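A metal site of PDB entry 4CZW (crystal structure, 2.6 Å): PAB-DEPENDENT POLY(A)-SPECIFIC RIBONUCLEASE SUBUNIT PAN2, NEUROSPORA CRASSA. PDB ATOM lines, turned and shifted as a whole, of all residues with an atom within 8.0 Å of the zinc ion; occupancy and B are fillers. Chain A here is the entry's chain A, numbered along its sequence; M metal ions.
O of His 70 is in hydrogen-bond range of OG1 of Thr 73 (2.6 Å).
The side-chain sulfur (SG) of Cys 83 sits close to the side-chain amino group (NZ) of Lys 530, at 3.5 Å.
NZ of Lys 530 lies within hydrogen-bond range of O of Cys 75, at 2.5 Å.
The backbone NH (N) of Ala 77 lies close to the side-chain sulfur (SG) of Cys 75, 3.6 Å away.
OG1 of Thr 73 sits close to N of Cys 75.
NZ of Lys 534 sits at hydrogen-bond distance from O of Cys 75, 3.3 Å away.
Within 4 Å of the zinc ion: His 70, Cys 75, Cys 80 and Cys 83.
The nearest printed residue that does not touch the zinc ion is Lys 530 (4.2 Å).
The zinc ion is bound by NE2 of His 70, SG of Cys 80, SG of Cys 83 and SG of Cys 75.
The zinc ion has four donor atoms within binding distance.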
ATOM      1  N   ALA A  67     -33.351  33.126  -2.620  1.00  0.00           N
ATOM      2  CA  ALA A  67     -32.500  32.053  -2.122  1.00  0.00           C
ATOM      3  C   ALA A  67     -32.628  30.792  -2.980  1.00  0.00           C
ATOM      4  O   ALA A  67     -31.630  30.131  -3.262  1.00  0.00           O
ATOM      5  CB  ALA A  67     -32.832  31.741  -0.676  1.00  0.00           C
ATOM      6  N   HIS A  70     -30.904  30.880  -6.357  1.00  0.00           N
ATOM      7  CA  HIS A  70     -29.459  30.730  -6.226  1.00  0.00           C
ATOM      8  C   HIS A  70     -29.067  29.300  -5.862  1.00  0.00           C
ATOM      9  O   HIS A  70     -28.127  28.745  -6.425  1.00  0.00           O
ATOM     10  CB  HIS A  70     -28.898  31.682  -5.166  1.00  0.00           C
ATOM     11  CG  HIS A  70     -27.466  31.426  -4.824  1.00  0.00           C
ATOM     12  ND1 HIS A  70     -26.426  31.752  -5.660  1.00  0.00           N
ATOM     13  CD2 HIS A  70     -26.900  30.848  -3.737  1.00  0.00           C
ATOM     14  CE1 HIS A  70     -25.282  31.407  -5.100  1.00  0.00           C
ATOM     15  NE2 HIS A  70     -25.547  30.844  -3.928  1.00  0.00           N
ATOM     16  N   ALA A  71     -29.784  28.716  -4.904  1.00  0.00           N
ATOM     17  CA  ALA A  71     -29.491  27.365  -4.431  1.00  0.00           C
ATOM     18  C   ALA A  71     -29.642  26.342  -5.554  1.00  0.00           C
ATOM     19  O   ALA A  71     -29.002  25.286  -5.533  1.00  0.00           O
ATOM     20  CB  ALA A  71     -30.391  27.007  -3.267  1.00  0.00           C
ATOM     21  N   ALA A  72     -30.487  26.648  -6.522  1.00  0.00           N
ATOM     22  CA  ALA A  72     -30.770  25.739  -7.627  1.00  0.00           C
ATOM     23  C   ALA A  72     -29.690  25.784  -8.709  1.00  0.00           C
ATOM     24  O   ALA A  72     -29.742  25.043  -9.683  1.00  0.00           O
ATOM     25  CB  ALA A  72     -32.123  26.057  -8.239  1.00  0.00           C
ATOM     26  N   THR A  73     -28.695  26.658  -8.526  1.00  0.00           N
ATOM     27  CA  THR A  73     -27.608  26.767  -9.484  1.00  0.00           C
ATOM     28  C   THR A  73     -26.518  25.732  -9.208  1.00  0.00           C
ATOM     29  O   THR A  73     -26.694  24.857  -8.358  1.00  0.00           O
ATOM     30  CB  THR A  73     -26.970  28.182  -9.477  1.00  0.00           C
ATOM     31  OG1 THR A  73     -26.274  28.386  -8.246  1.00  0.00           O
ATOM     32  CG2 THR A  73     -28.045  29.241  -9.646  1.00  0.00           C
ATOM     33  N   ALA A  74     -25.409  25.847  -9.915  1.00  0.00           N
ATOM     34  CA  ALA A  74     -24.303  24.904  -9.767  1.00  0.00           C
ATOM     35  C   ALA A  74     -23.316  25.351  -8.694  1.00  0.00           C
ATOM     36  O   ALA A  74     -22.196  24.845  -8.629  1.00  0.00           O
ATOM     37  CB  ALA A  74     -23.588  24.713 -11.100  1.00  0.00           C
ATOM     38  N   CYS A  75     -23.748  26.301  -7.866  1.00  0.00           N
ATOM     39  CA  CYS A  75     -22.903  26.865  -6.814  1.00  0.00           C
ATOM     40  C   CYS A  75     -22.333  25.785  -5.895  1.00  0.00           C
ATOM     41  O   CYS A  75     -23.068  25.056  -5.242  1.00  0.00           O
ATOM     42  CB  CYS A  75     -23.691  27.878  -5.983  1.00  0.00           C
ATOM     43  SG  CYS A  75     -22.797  28.592  -4.581  1.00  0.00           S
ATOM     44  N   LEU A  76     -21.006  25.692  -5.864  1.00  0.00           N
ATOM     45  CA  LEU A  76     -20.318  24.724  -5.022  1.00  0.00           C
ATOM     46  C   LEU A  76     -19.566  25.421  -3.890  1.00  0.00           C
ATOM     47  O   LEU A  76     -18.666  24.842  -3.284  1.00  0.00           O
ATOM     48  CB  LEU A  76     -19.347  23.874  -5.848  1.00  0.00           C
ATOM     49  CG  LEU A  76     -19.974  22.922  -6.864  1.00  0.00           C
ATOM     50  CD1 LEU A  76     -18.895  22.159  -7.608  1.00  0.00           C
ATOM     51  CD2 LEU A  76     -20.923  21.958  -6.171  1.00  0.00           C
ATOM     52  N   ALA A  77     -19.954  26.665  -3.613  1.00  0.00           N
ATOM     53  CA  ALA A  77     -19.342  27.425  -2.526  1.00  0.00           C
ATOM     54  C   ALA A  77     -19.741  26.837  -1.174  1.00  0.00           C
ATOM     55  O   ALA A  77     -20.912  26.526  -0.941  1.00  0.00           O
ATOM     56  CB  ALA A  77     -19.735  28.886  -2.607  1.00  0.00           C
ATOM     57  N   ASP A  78     -18.762  26.680  -0.292  1.00  0.00           N
ATOM     58  CA  ASP A  78     -19.008  26.135   1.038  1.00  0.00           C
ATOM     59  C   ASP A  78     -17.953  26.663   2.006  1.00  0.00           C
ATOM     60  O   ASP A  78     -16.766  26.377   1.843  1.00  0.00           O
ATOM     61  CB  ASP A  78     -18.995  24.602   1.002  1.00  0.00           C
ATOM     62  CG  ASP A  78     -19.425  23.989   2.322  1.00  0.00           C
ATOM     63  OD1 ASP A  78     -20.213  24.621   3.053  1.00  0.00           O
ATOM     64  OD2 ASP A  78     -18.967  22.866   2.632  1.00  0.00           O
ATOM     65  N   PRO A  79     -18.388  27.433   3.023  1.00  0.00           N
ATOM     66  CA  PRO A  79     -19.780  27.763   3.350  1.00  0.00           C
ATOM     67  C   PRO A  79     -20.408  28.810   2.415  1.00  0.00           C
ATOM     68  O   PRO A  79     -19.714  29.660   1.855  1.00  0.00           O
ATOM     69  CB  PRO A  79     -19.672  28.323   4.771  1.00  0.00           C
ATOM     70  CG  PRO A  79     -18.317  28.913   4.825  1.00  0.00           C
ATOM     71  CD  PRO A  79     -17.444  28.007   4.005  1.00  0.00           C
ATOM     72  N   CYS A  80     -21.729  28.716   2.265  1.00  0.00           N
ATOM     73  CA  CYS A  80     -22.495  29.635   1.434  1.00  0.00           C
ATOM     74  C   CYS A  80     -23.893  29.792   2.042  1.00  0.00           C
ATOM     75  O   CYS A  80     -24.771  28.957   1.813  1.00  0.00           O
ATOM     76  CB  CYS A  80     -22.583  29.136   0.002  1.00  0.00           C
ATOM     77  SG  CYS A  80     -23.541  30.166  -1.128  1.00  0.00           S
ATOM     78  N   LEU A  81     -24.082  30.867   2.799  1.00  0.00           N
ATOM     79  CA  LEU A  81     -25.295  31.052   3.596  1.00  0.00           C
ATOM     80  C   LEU A  81     -26.561  31.182   2.748  1.00  0.00           C
ATOM     81  O   LEU A  81     -27.641  30.814   3.198  1.00  0.00           O
ATOM     82  CB  LEU A  81     -25.143  32.292   4.483  1.00  0.00           C
ATOM     83  CG  LEU A  81     -24.031  32.207   5.536  1.00  0.00           C
ATOM     84  CD1 LEU A  81     -24.000  33.464   6.392  1.00  0.00           C
ATOM     85  CD2 LEU A  81     -24.195  30.964   6.404  1.00  0.00           C
ATOM     86  N   LEU A  82     -26.432  31.704   1.535  1.00  0.00           N
ATOM     87  CA  LEU A  82     -27.581  31.852   0.654  1.00  0.00           C
ATOM     88  C   LEU A  82     -28.085  30.495   0.184  1.00  0.00           C
ATOM     89  O   LEU A  82     -29.284  30.266   0.082  1.00  0.00           O
ATOM     90  CB  LEU A  82     -27.251  32.748  -0.534  1.00  0.00           C
ATOM     91  CG  LEU A  82     -28.440  33.093  -1.435  1.00  0.00           C
ATOM     92  CD1 LEU A  82     -29.578  33.669  -0.614  1.00  0.00           C
ATOM     93  CD2 LEU A  82     -28.018  34.072  -2.518  1.00  0.00           C
ATOM     94  N   CYS A  83     -27.150  29.596  -0.115  1.00  0.00           N
ATOM     95  CA  CYS A  83     -27.501  28.217  -0.466  1.00  0.00           C
ATOM     96  C   CYS A  83     -28.177  27.537   0.713  1.00  0.00           C
ATOM     97  O   CYS A  83     -29.198  26.879   0.556  1.00  0.00           O
ATOM     98  CB  CYS A  83     -26.256  27.431  -0.898  1.00  0.00           C
ATOM     99  SG  CYS A  83     -25.836  27.603  -2.648  1.00  0.00           S
ATOM    100  N   GLU A  84     -27.588  27.698   1.887  1.00  0.00           N
ATOM    101  CA  GLU A  84     -28.142  27.130   3.111  1.00  0.00           C
ATOM    102  C   GLU A  84     -29.512  27.722   3.408  1.00  0.00           C
ATOM    103  O   GLU A  84     -30.391  27.037   3.927  1.00  0.00           O
ATOM    104  CB  GLU A  84     -27.192  27.379   4.290  1.00  0.00           C
ATOM    105  CG  GLU A  84     -25.793  26.805   4.099  1.00  0.00           C
ATOM    106  CD  GLU A  84     -25.790  25.281   4.084  1.00  0.00           C
ATOM    107  OE1 GLU A  84     -26.701  24.675   4.680  1.00  0.00           O
ATOM    108  OE2 GLU A  84     -24.859  24.699   3.485  1.00  0.00           O
ATOM    109  N   TYR A  87     -31.978  25.896   1.304  1.00  0.00           N
ATOM    110  CA  TYR A  87     -32.236  24.565   1.862  1.00  0.00           C
ATOM    111  C   TYR A  87     -33.262  24.638   2.979  1.00  0.00           C
ATOM    112  O   TYR A  87     -34.199  23.845   3.032  1.00  0.00           O
ATOM    113  CB  TYR A  87     -30.936  23.933   2.383  1.00  0.00           C
ATOM    114  CG  TYR A  87     -29.850  23.802   1.346  1.00  0.00           C
ATOM    115  CD1 TYR A  87     -30.155  23.698  -0.011  1.00  0.00           C
ATOM    116  CD2 TYR A  87     -28.508  23.792   1.712  1.00  0.00           C
ATOM    117  CE1 TYR A  87     -29.159  23.573  -0.961  1.00  0.00           C
ATOM    118  CE2 TYR A  87     -27.511  23.668   0.771  1.00  0.00           C
ATOM    119  CZ  TYR A  87     -27.830  23.560  -0.562  1.00  0.00           C
ATOM    120  OH  TYR A  87     -26.836  23.446  -1.503  1.00  0.00           O
ATOM    121  N   ASP A 148     -23.385  36.685  -2.254  1.00  0.00           N
ATOM    122  CA  ASP A 148     -23.556  35.293  -2.646  1.00  0.00           C
ATOM    123  C   ASP A 148     -24.429  35.216  -3.893  1.00  0.00           C
ATOM    124  O   ASP A 148     -24.223  34.364  -4.756  1.00  0.00           O
ATOM    125  CB  ASP A 148     -24.177  34.480  -1.519  1.00  0.00           C
ATOM    126  CG  ASP A 148     -23.196  34.149  -0.419  1.00  0.00           C
ATOM    127  OD1 ASP A 148     -21.970  34.190  -0.675  1.00  0.00           O
ATOM    128  OD2 ASP A 148     -23.638  33.848   0.707  1.00  0.00           O
ATOM    129  N   TYR A 149     -25.413  36.101  -3.973  1.00  0.00           N
ATOM    130  CA  TYR A 149     -26.370  36.111  -5.074  1.00  0.00           C
ATOM    131  C   TYR A 149     -25.708  36.487  -6.404  1.00  0.00           C
ATOM    132  O   TYR A 149     -26.094  36.003  -7.457  1.00  0.00           O
ATOM    133  CB  TYR A 149     -27.518  37.072  -4.766  1.00  0.00           C
ATOM    134  CG  TYR A 149     -28.599  37.126  -5.820  1.00  0.00           C
ATOM    135  CD1 TYR A 149     -29.632  36.197  -5.825  1.00  0.00           C
ATOM    136  CD2 TYR A 149     -28.586  38.102  -6.809  1.00  0.00           C
ATOM    137  CE1 TYR A 149     -30.622  36.237  -6.791  1.00  0.00           C
ATOM    138  CE2 TYR A 149     -29.569  38.155  -7.768  1.00  0.00           C
ATOM    139  CZ  TYR A 149     -30.588  37.222  -7.764  1.00  0.00           C
ATOM    140  OH  TYR A 149     -31.580  37.273  -8.721  1.00  0.00           O
ATOM    141  N   GLY A 151     -22.500  36.044  -7.051  1.00  0.00           N
ATOM    142  CA  GLY A 151     -21.375  35.164  -7.294  1.00  0.00           C
ATOM    143  C   GLY A 151     -21.559  34.313  -8.538  1.00  0.00           C
ATOM    144  O   GLY A 151     -20.644  34.149  -9.335  1.00  0.00           O
ATOM    145  N   THR A 152     -22.767  33.790  -8.700  1.00  0.00           N
ATOM    146  CA  THR A 152     -23.119  32.999  -9.881  1.00  0.00           C
ATOM    147  C   THR A 152     -24.527  33.363 -10.335  1.00  0.00           C
ATOM    148  O   THR A 152     -25.411  33.583  -9.510  1.00  0.00           O
ATOM    149  CB  THR A 152     -23.026  31.477  -9.594  1.00  0.00           C
ATOM    150  OG1 THR A 152     -23.548  30.747 -10.712  1.00  0.00           O
ATOM    151  CG2 THR A 152     -23.807  31.116  -8.338  1.00  0.00           C
ATOM    152  N   LYS A 530     -21.568  20.510   2.225  1.00  0.00           N
ATOM    153  CA  LYS A 530     -22.568  21.106   1.347  1.00  0.00           C
ATOM    154  C   LYS A 530     -22.524  20.497  -0.053  1.00  0.00           C
ATOM    155  O   LYS A 530     -23.539  20.441  -0.745  1.00  0.00           O
ATOM    156  CB  LYS A 530     -22.363  22.625   1.274  1.00  0.00           C
ATOM    157  CG  LYS A 530     -23.392  23.375   0.453  1.00  0.00           C
ATOM    158  CD  LYS A 530     -22.804  23.886  -0.852  1.00  0.00           C
ATOM    159  CE  LYS A 530     -23.772  24.793  -1.593  1.00  0.00           C
ATOM    160  NZ  LYS A 530     -23.154  25.408  -2.794  1.00  0.00           N
ATOM    161  N   LYS A 534     -25.754  18.854  -1.574  1.00  0.00           N
ATOM    162  CA  LYS A 534     -26.268  19.428  -2.822  1.00  0.00           C
ATOM    163  C   LYS A 534     -26.791  18.329  -3.745  1.00  0.00           C
ATOM    164  O   LYS A 534     -27.823  18.504  -4.405  1.00  0.00           O
ATOM    165  CB  LYS A 534     -25.183  20.238  -3.529  1.00  0.00           C
ATOM    166  CG  LYS A 534     -25.666  21.041  -4.723  1.00  0.00           C
ATOM    167  CD  LYS A 534     -24.526  21.789  -5.379  1.00  0.00           C
ATOM    168  CE  LYS A 534     -25.005  22.628  -6.548  1.00  0.00           C
ATOM    169  NZ  LYS A 534     -25.912  23.728  -6.107  1.00  0.00           N
HETATM  170 ZN    ZN M   1     -24.418  29.373  -3.096  1.00  0.00          ZN
